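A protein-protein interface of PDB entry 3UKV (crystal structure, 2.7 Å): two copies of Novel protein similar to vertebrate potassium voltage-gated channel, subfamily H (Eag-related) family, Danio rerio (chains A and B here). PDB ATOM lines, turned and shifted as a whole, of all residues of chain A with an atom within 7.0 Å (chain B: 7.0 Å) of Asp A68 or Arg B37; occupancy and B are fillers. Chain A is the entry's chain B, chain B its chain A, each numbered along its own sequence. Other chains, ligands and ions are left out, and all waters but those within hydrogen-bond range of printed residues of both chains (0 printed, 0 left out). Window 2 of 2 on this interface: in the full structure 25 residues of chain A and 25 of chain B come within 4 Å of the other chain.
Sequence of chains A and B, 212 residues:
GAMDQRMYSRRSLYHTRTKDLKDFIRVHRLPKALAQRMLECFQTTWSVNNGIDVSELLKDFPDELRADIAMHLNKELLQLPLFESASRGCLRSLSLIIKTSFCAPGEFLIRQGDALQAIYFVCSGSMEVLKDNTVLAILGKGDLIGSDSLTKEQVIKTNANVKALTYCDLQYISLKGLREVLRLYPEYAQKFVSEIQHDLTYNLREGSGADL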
ATOM      1  N   PHE A  61      -5.313 -22.346  -2.909  1.00  0.00           N
ATOM      2  CA  PHE A  61      -4.853 -20.982  -3.038  1.00  0.00           C
ATOM      3  C   PHE A  61      -3.741 -20.950  -4.071  1.00  0.00           C
ATOM      4  O   PHE A  61      -3.013 -21.927  -4.225  1.00  0.00           O
ATOM      5  CB  PHE A  61      -4.367 -20.430  -1.698  1.00  0.00           C
ATOM      6  CG  PHE A  61      -5.477 -20.075  -0.731  1.00  0.00           C
ATOM      7  CD1 PHE A  61      -6.756 -20.552  -0.898  1.00  0.00           C
ATOM      8  CD2 PHE A  61      -5.233 -19.247   0.346  1.00  0.00           C
ATOM      9  CE1 PHE A  61      -7.753 -20.211   0.003  1.00  0.00           C
ATOM     10  CE2 PHE A  61      -6.246 -18.901   1.240  1.00  0.00           C
ATOM     11  CZ  PHE A  61      -7.483 -19.376   1.072  1.00  0.00           C
ATOM     12  N   ASP A  63      -0.185 -20.063  -5.820  1.00  0.00           N
ATOM     13  CA  ASP A  63       1.119 -20.217  -5.186  1.00  0.00           C
ATOM     14  C   ASP A  63       1.685 -18.922  -4.590  1.00  0.00           C
ATOM     15  O   ASP A  63       2.455 -18.972  -3.631  1.00  0.00           O
ATOM     16  CB  ASP A  63       2.124 -20.839  -6.156  1.00  0.00           C
ATOM     17  CG  ASP A  63       1.728 -22.243  -6.591  1.00  0.00           C
ATOM     18  OD1 ASP A  63       1.284 -23.047  -5.730  1.00  0.00           O
ATOM     19  OD2 ASP A  63       1.870 -22.534  -7.803  1.00  0.00           O
ATOM     20  N   GLU A  64       1.316 -17.767  -5.136  1.00  0.00           N
ATOM     21  CA  GLU A  64       1.812 -16.524  -4.549  1.00  0.00           C
ATOM     22  C   GLU A  64       1.236 -16.316  -3.166  1.00  0.00           C
ATOM     23  O   GLU A  64       1.962 -15.918  -2.240  1.00  0.00           O
ATOM     24  CB  GLU A  64       1.513 -15.300  -5.407  1.00  0.00           C
ATOM     25  CG  GLU A  64       2.301 -15.224  -6.704  1.00  0.00           C
ATOM     26  CD  GLU A  64       1.594 -15.894  -7.873  1.00  0.00           C
ATOM     27  OE1 GLU A  64       2.237 -16.063  -8.932  1.00  0.00           O
ATOM     28  OE2 GLU A  64       0.402 -16.240  -7.731  1.00  0.00           O
ATOM     29  N   LEU A  65      -0.063 -16.589  -3.017  1.00  0.00           N
ATOM     30  CA  LEU A  65      -0.714 -16.421  -1.718  1.00  0.00           C
ATOM     31  C   LEU A  65      -0.181 -17.444  -0.743  1.00  0.00           C
ATOM     32  O   LEU A  65       0.084 -17.137   0.409  1.00  0.00           O
ATOM     33  CB  LEU A  65      -2.226 -16.540  -1.816  1.00  0.00           C
ATOM     34  CG  LEU A  65      -2.995 -15.956  -0.634  1.00  0.00           C
ATOM     35  CD1 LEU A  65      -2.538 -14.538  -0.266  1.00  0.00           C
ATOM     36  CD2 LEU A  65      -4.468 -15.974  -0.969  1.00  0.00           C
ATOM     37  N   ARG A  66      -0.003 -18.664  -1.219  1.00  0.00           N
ATOM     38  CA  ARG A  66       0.583 -19.679  -0.382  1.00  0.00           C
ATOM     39  C   ARG A  66       1.969 -19.239   0.119  1.00  0.00           C
ATOM     40  O   ARG A  66       2.275 -19.402   1.304  1.00  0.00           O
ATOM     41  CB  ARG A  66       0.610 -21.046  -1.086  1.00  0.00           C
ATOM     42  CG  ARG A  66      -0.770 -21.665  -1.277  1.00  0.00           C
ATOM     43  CD  ARG A  66      -0.739 -22.893  -2.168  1.00  0.00           C
ATOM     44  NE  ARG A  66       0.196 -23.908  -1.694  1.00  0.00           N
ATOM     45  CZ  ARG A  66      -0.117 -24.855  -0.813  1.00  0.00           C
ATOM     46  NH1 ARG A  66      -1.334 -24.908  -0.293  1.00  0.00           N
ATOM     47  NH2 ARG A  66       0.782 -25.744  -0.438  1.00  0.00           N
ATOM     48  N   ALA A  67       2.805 -18.675  -0.746  1.00  0.00           N
ATOM     49  CA  ALA A  67       4.146 -18.259  -0.300  1.00  0.00           C
ATOM     50  C   ALA A  67       4.088 -17.135   0.766  1.00  0.00           C
ATOM     51  O   ALA A  67       4.821 -17.184   1.758  1.00  0.00           O
ATOM     52  CB  ALA A  67       5.021 -17.850  -1.480  1.00  0.00           C
ATOM     53  N   ASP A  68       3.218 -16.144   0.554  1.00  0.00           N
ATOM     54  CA  ASP A  68       3.078 -15.049   1.488  1.00  0.00           C
ATOM     55  C   ASP A  68       2.609 -15.593   2.832  1.00  0.00           C
ATOM     56  O   ASP A  68       3.141 -15.221   3.887  1.00  0.00           O
ATOM     57  CB  ASP A  68       2.101 -13.998   0.974  1.00  0.00           C
ATOM     58  CG  ASP A  68       2.621 -13.247  -0.239  1.00  0.00           C
ATOM     59  OD1 ASP A  68       3.844 -13.258  -0.497  1.00  0.00           O
ATOM     60  OD2 ASP A  68       1.795 -12.633  -0.939  1.00  0.00           O
ATOM     61  N   ILE A  69       1.624 -16.483   2.810  1.00  0.00           N
ATOM     62  CA  ILE A  69       1.203 -17.109   4.051  1.00  0.00           C
ATOM     63  C   ILE A  69       2.376 -17.841   4.713  1.00  0.00           C
ATOM     64  O   ILE A  69       2.732 -17.538   5.838  1.00  0.00           O
ATOM     65  CB  ILE A  69       0.035 -18.092   3.859  1.00  0.00           C
ATOM     66  CG1 ILE A  69      -1.183 -17.378   3.284  1.00  0.00           C
ATOM     67  CG2 ILE A  69      -0.298 -18.760   5.184  1.00  0.00           C
ATOM     68  CD1 ILE A  69      -2.297 -18.294   2.882  1.00  0.00           C
ATOM     69  N   ALA A  70       2.968 -18.808   4.024  1.00  0.00           N
ATOM     70  CA  ALA A  70       4.074 -19.581   4.582  1.00  0.00           C
ATOM     71  C   ALA A  70       5.158 -18.715   5.210  1.00  0.00           C
ATOM     72  O   ALA A  70       5.718 -19.060   6.255  1.00  0.00           O
ATOM     73  CB  ALA A  70       4.687 -20.489   3.516  1.00  0.00           C
ATOM     74  N   MET A  71       5.453 -17.601   4.551  1.00  0.00           N
ATOM     75  CA  MET A  71       6.496 -16.663   4.951  1.00  0.00           C
ATOM     76  C   MET A  71       6.334 -16.151   6.376  1.00  0.00           C
ATOM     77  O   MET A  71       7.271 -15.611   6.964  1.00  0.00           O
ATOM     78  CB  MET A  71       6.440 -15.461   4.013  1.00  0.00           C
ATOM     79  CG  MET A  71       7.733 -15.140   3.339  1.00  0.00           C
ATOM     80  SD  MET A  71       7.546 -13.665   2.339  1.00  0.00           S
ATOM     81  CE  MET A  71       6.444 -14.250   1.040  1.00  0.00           C
ATOM     82  N   HIS A  72       5.124 -16.286   6.908  1.00  0.00           N
ATOM     83  CA  HIS A  72       4.764 -15.732   8.208  1.00  0.00           C
ATOM     84  C   HIS A  72       4.740 -16.800   9.290  1.00  0.00           C
ATOM     85  O   HIS A  72       4.396 -16.536  10.444  1.00  0.00           O
ATOM     86  CB  HIS A  72       3.387 -15.086   8.130  1.00  0.00           C
ATOM     87  CG  HIS A  72       3.414 -13.653   7.716  1.00  0.00           C
ATOM     88  ND1 HIS A  72       3.512 -13.259   6.400  1.00  0.00           N
ATOM     89  CD2 HIS A  72       3.354 -12.515   8.446  1.00  0.00           C
ATOM     90  CE1 HIS A  72       3.507 -11.940   6.336  1.00  0.00           C
ATOM     91  NE2 HIS A  72       3.410 -11.464   7.565  1.00  0.00           N
ATOM     92  N   LEU A  73       5.064 -18.021   8.910  1.00  0.00           N
ATOM     93  CA  LEU A  73       4.948 -19.127   9.835  1.00  0.00           C
ATOM     94  C   LEU A  73       6.344 -19.533  10.202  1.00  0.00           C
ATOM     95  O   LEU A  73       7.257 -19.434   9.384  1.00  0.00           O
ATOM     96  CB  LEU A  73       4.235 -20.315   9.194  1.00  0.00           C
ATOM     97  CG  LEU A  73       2.864 -20.117   8.578  1.00  0.00           C
ATOM     98  CD1 LEU A  73       2.279 -21.469   8.266  1.00  0.00           C
ATOM     99  CD2 LEU A  73       1.948 -19.373   9.511  1.00  0.00           C
ATOM    100  N   ARG A  92       7.835 -24.855   2.802  1.00  0.00           N
ATOM    101  CA  ARG A  92       6.609 -24.061   2.727  1.00  0.00           C
ATOM    102  C   ARG A  92       5.355 -24.948   2.683  1.00  0.00           C
ATOM    103  O   ARG A  92       4.345 -24.657   3.316  1.00  0.00           O
ATOM    104  CB  ARG A  92       6.634 -23.116   1.520  1.00  0.00           C
ATOM    105  CG  ARG A  92       5.270 -22.999   0.778  1.00  0.00           C
ATOM    106  CD  ARG A  92       5.449 -22.690  -0.724  1.00  0.00           C
ATOM    107  NE  ARG A  92       6.493 -21.687  -0.790  1.00  0.00           N
ATOM    108  CZ  ARG A  92       7.178 -21.358  -1.883  1.00  0.00           C
ATOM    109  NH1 ARG A  92       6.899 -21.961  -3.050  1.00  0.00           N
ATOM    110  NH2 ARG A  92       8.137 -20.411  -1.791  1.00  0.00           N
ATOM    111  N   LEU B  30      -1.529 -12.957  11.533  1.00  0.00           N
ATOM    112  CA  LEU B  30      -1.263 -12.565  10.133  1.00  0.00           C
ATOM    113  C   LEU B  30      -1.784 -11.185   9.831  1.00  0.00           C
ATOM    114  O   LEU B  30      -2.884 -10.824  10.241  1.00  0.00           O
ATOM    115  CB  LEU B  30      -1.914 -13.524   9.152  1.00  0.00           C
ATOM    116  CG  LEU B  30      -1.387 -14.946   9.167  1.00  0.00           C
ATOM    117  CD1 LEU B  30      -1.923 -15.680   7.959  1.00  0.00           C
ATOM    118  CD2 LEU B  30       0.125 -14.932   9.161  1.00  0.00           C
ATOM    119  N   PRO B  31      -0.989 -10.411   9.096  1.00  0.00           N
ATOM    120  CA  PRO B  31      -1.265  -9.016   8.757  1.00  0.00           C
ATOM    121  C   PRO B  31      -2.629  -8.817   8.084  1.00  0.00           C
ATOM    122  O   PRO B  31      -3.005  -9.588   7.196  1.00  0.00           O
ATOM    123  CB  PRO B  31      -0.137  -8.664   7.782  1.00  0.00           C
ATOM    124  CG  PRO B  31       0.966  -9.601   8.094  1.00  0.00           C
ATOM    125  CD  PRO B  31       0.310 -10.869   8.574  1.00  0.00           C
ATOM    126  N   LYS B  32      -3.343  -7.780   8.509  1.00  0.00           N
ATOM    127  CA  LYS B  32      -4.657  -7.450   8.001  1.00  0.00           C
ATOM    128  C   LYS B  32      -4.747  -7.499   6.476  1.00  0.00           C
ATOM    129  O   LYS B  32      -5.745  -7.988   5.932  1.00  0.00           O
ATOM    130  CB  LYS B  32      -5.055  -6.064   8.503  1.00  0.00           C
ATOM    131  CG  LYS B  32      -5.075  -5.931  10.033  1.00  0.00           C
ATOM    132  CD  LYS B  32      -6.420  -6.353  10.616  1.00  0.00           C
ATOM    133  CE  LYS B  32      -6.297  -6.655  12.079  1.00  0.00           C
ATOM    134  NZ  LYS B  32      -7.593  -7.119  12.641  1.00  0.00           N
ATOM    135  N   ALA B  33      -3.715  -6.995   5.795  1.00  0.00           N
ATOM    136  CA  ALA B  33      -3.659  -7.029   4.328  1.00  0.00           C
ATOM    137  C   ALA B  33      -3.639  -8.450   3.753  1.00  0.00           C
ATOM    138  O   ALA B  33      -4.413  -8.777   2.840  1.00  0.00           O
ATOM    139  CB  ALA B  33      -2.466  -6.249   3.824  1.00  0.00           C
ATOM    140  N   LEU B  34      -2.741  -9.280   4.281  1.00  0.00           N
ATOM    141  CA  LEU B  34      -2.718 -10.698   3.955  1.00  0.00           C
ATOM    142  C   LEU B  34      -4.024 -11.383   4.400  1.00  0.00           C
ATOM    143  O   LEU B  34      -4.615 -12.140   3.649  1.00  0.00           O
ATOM    144  CB  LEU B  34      -1.506 -11.385   4.589  1.00  0.00           C
ATOM    145  CG  LEU B  34      -1.265 -12.819   4.117  1.00  0.00           C
ATOM    146  CD1 LEU B  34      -0.955 -12.844   2.656  1.00  0.00           C
ATOM    147  CD2 LEU B  34      -0.136 -13.445   4.850  1.00  0.00           C
ATOM    148  N   ALA B  35      -4.497 -11.107   5.609  1.00  0.00           N
ATOM    149  CA  ALA B  35      -5.795 -11.641   6.012  1.00  0.00           C
ATOM    150  C   ALA B  35      -6.861 -11.376   4.938  1.00  0.00           C
ATOM    151  O   ALA B  35      -7.668 -12.240   4.621  1.00  0.00           O
ATOM    152  CB  ALA B  35      -6.216 -11.048   7.309  1.00  0.00           C
ATOM    153  N   GLN B  36      -6.843 -10.178   4.370  1.00  0.00           N
ATOM    154  CA  GLN B  36      -7.869  -9.751   3.430  1.00  0.00           C
ATOM    155  C   GLN B  36      -7.786 -10.536   2.111  1.00  0.00           C
ATOM    156  O   GLN B  36      -8.807 -11.034   1.592  1.00  0.00           O
ATOM    157  CB  GLN B  36      -7.767  -8.244   3.177  1.00  0.00           C
ATOM    158  CG  GLN B  36      -9.022  -7.632   2.561  1.00  0.00           C
ATOM    159  CD  GLN B  36     -10.309  -8.012   3.315  1.00  0.00           C
ATOM    160  OE1 GLN B  36     -11.080  -8.881   2.878  1.00  0.00           O
ATOM    161  NE2 GLN B  36     -10.546  -7.350   4.450  1.00  0.00           N
ATOM    162  N   ARG B  37      -6.570 -10.651   1.581  1.00  0.00           N
ATOM    163  CA  ARG B  37      -6.335 -11.486   0.423  1.00  0.00           C
ATOM    164  C   ARG B  37      -6.783 -12.941   0.667  1.00  0.00           C
ATOM    165  O   ARG B  37      -7.437 -13.551  -0.183  1.00  0.00           O
ATOM    166  CB  ARG B  37      -4.865 -11.423   0.017  1.00  0.00           C
ATOM    167  CG  ARG B  37      -4.417 -10.053  -0.427  1.00  0.00           C
ATOM    168  CD  ARG B  37      -2.911  -9.975  -0.456  1.00  0.00           C
ATOM    169  NE  ARG B  37      -2.359 -11.053  -1.272  1.00  0.00           N
ATOM    170  CZ  ARG B  37      -1.105 -11.480  -1.191  1.00  0.00           C
ATOM    171  NH1 ARG B  37      -0.269 -10.926  -0.309  1.00  0.00           N
ATOM    172  NH2 ARG B  37      -0.697 -12.468  -1.979  1.00  0.00           N
ATOM    173  N   MET B  38      -6.451 -13.486   1.831  1.00  0.00           N
ATOM    174  CA  MET B  38      -6.886 -14.823   2.163  1.00  0.00           C
ATOM    175  C   MET B  38      -8.417 -15.037   2.137  1.00  0.00           C
ATOM    176  O   MET B  38      -8.908 -16.080   1.700  1.00  0.00           O
ATOM    177  CB  MET B  38      -6.330 -15.215   3.513  1.00  0.00           C
ATOM    178  CG  MET B  38      -4.853 -15.282   3.536  1.00  0.00           C
ATOM    179  SD  MET B  38      -4.280 -15.673   5.203  1.00  0.00           S
ATOM    180  CE  MET B  38      -4.661 -17.432   5.229  1.00  0.00           C
ATOM    181  N   LEU B  39      -9.162 -14.058   2.627  1.00  0.00           N
ATOM    182  CA  LEU B  39     -10.597 -14.198   2.768  1.00  0.00           C
ATOM    183  C   LEU B  39     -11.292 -14.049   1.430  1.00  0.00           C
ATOM    184  O   LEU B  39     -12.264 -14.741   1.143  1.00  0.00           O
ATOM    185  CB  LEU B  39     -11.131 -13.181   3.798  1.00  0.00           C
ATOM    186  CG  LEU B  39     -10.956 -13.713   5.234  1.00  0.00           C
ATOM    187  CD1 LEU B  39     -10.814 -12.624   6.284  1.00  0.00           C
ATOM    188  CD2 LEU B  39     -12.068 -14.695   5.604  1.00  0.00           C
ATOM    189  N   GLU B  40     -10.770 -13.132   0.621  1.00  0.00           N
ATOM    190  CA  GLU B  40     -11.281 -12.874  -0.714  1.00  0.00           C
ATOM    191  C   GLU B  40     -11.077 -14.086  -1.609  1.00  0.00           C
ATOM    192  O   GLU B  40     -11.991 -14.546  -2.287  1.00  0.00           O
ATOM    193  CB  GLU B  40     -10.578 -11.662  -1.296  1.00  0.00           C
ATOM    194  CG  GLU B  40     -10.772 -10.428  -0.464  1.00  0.00           C
ATOM    195  CD  GLU B  40     -10.928  -9.190  -1.311  1.00  0.00           C
ATOM    196  OE1 GLU B  40     -10.788  -9.308  -2.546  1.00  0.00           O
ATOM    197  OE2 GLU B  40     -11.201  -8.107  -0.748  1.00  0.00           O
ATOM    198  N   CYS B  41      -9.865 -14.613  -1.595  1.00  0.00           N
ATOM    199  CA  CYS B  41      -9.570 -15.803  -2.353  1.00  0.00           C
ATOM    200  C   CYS B  41     -10.290 -17.002  -1.761  1.00  0.00           C
ATOM    201  O   CYS B  41     -10.394 -18.043  -2.390  1.00  0.00           O
ATOM    202  CB  CYS B  41      -8.066 -16.048  -2.414  1.00  0.00           C
ATOM    203  SG  CYS B  41      -7.617 -17.600  -3.180  1.00  0.00           S
ATOM    204  N   PHE B  42     -10.812 -16.879  -0.554  1.00  0.00           N
ATOM    205  CA  PHE B  42     -11.567 -18.004  -0.053  1.00  0.00           C
ATOM    206  C   PHE B  42     -12.935 -18.086  -0.710  1.00  0.00           C
ATOM    207  O   PHE B  42     -13.346 -19.154  -1.135  1.00  0.00           O
ATOM    208  CB  PHE B  42     -11.718 -17.958   1.451  1.00  0.00           C
ATOM    209  CG  PHE B  42     -12.546 -19.076   2.003  1.00  0.00           C
ATOM    210  CD1 PHE B  42     -11.962 -20.283   2.336  1.00  0.00           C
ATOM    211  CD2 PHE B  42     -13.909 -18.920   2.182  1.00  0.00           C
ATOM    212  CE1 PHE B  42     -12.728 -21.315   2.853  1.00  0.00           C
ATOM    213  CE2 PHE B  42     -14.661 -19.934   2.684  1.00  0.00           C
ATOM    214  CZ  PHE B  42     -14.068 -21.138   3.030  1.00  0.00           C
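Among the printed residues, merely in contact across the chains: Phe A61 with Met B38, Phe A61 with Cys B41, Leu A65 with Leu B34, Leu A65 with Arg B37, Leu A65 with Cys B41, Asp A68 with Leu B34, Ile A69 with Leu B34, Ile A69 with Met B38, His A72 with Leu B30, His A72 with Pro B31 and His A72 with Leu B34.
Of chain A, only Leu A65 (3.3 Å) and Asp A68 (2.7 Å) come within 4 Å of Arg B37.
Of the printed residues of chain B, Phe A61 touches Met B38 (3.6 Å) and Cys B41 (3.8 Å).
Printed residues of chain B within 4 Å of Ile A69: Leu B34 and Met B38.
Of the printed residues of chain A, Pro B31 touches His A72 (3.1 Å).
Of the printed residues of chain A, Leu B30 touches His A72.
Of the printed residues of chain A, Met B38 touches Phe A61 and Ile A69.
Ala A70 touches none of the printed residues of chain B.
Leu A73 touches none of the printed residues of chain B.
The nearest residue of chain A that does not touch Arg B37 is Glu A64 (4.4 Å).
The nearest printed residue of chain B that does not touch Leu A65 is Met B38 (4.1 Å).
O of Asp A68 sits at hydrogen-bond distance from ND1 of His A72, at 3.2 Å.
No position is printed for both chains.
Of the 12 pairs that touch across the chains among the printed residues, none has its exchanged pair printed and touching as well.
Of the 13 printed residues of chain A, 5 touch a printed residue of chain B.
Hydrophobic or aromatic side chains of chain A that line the printed part of chain B: Phe A61, Leu A65, Ile A69 and His A72.
Printed residues of chain B that touch a printed residue of chain A: Leu B30, Pro B31, Leu B34, Arg B37, Met B38 and Cys B41.
Hydrophobic or aromatic side chains of chain B that line the printed part of chain A: Leu B30, Pro B31, Leu B34 and Met B38.
The guanidinium group (NH2) of Arg B37 is in salt-bridge range of the side-chain carboxylate (OD2) of Asp A68, 2.7 Å away.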
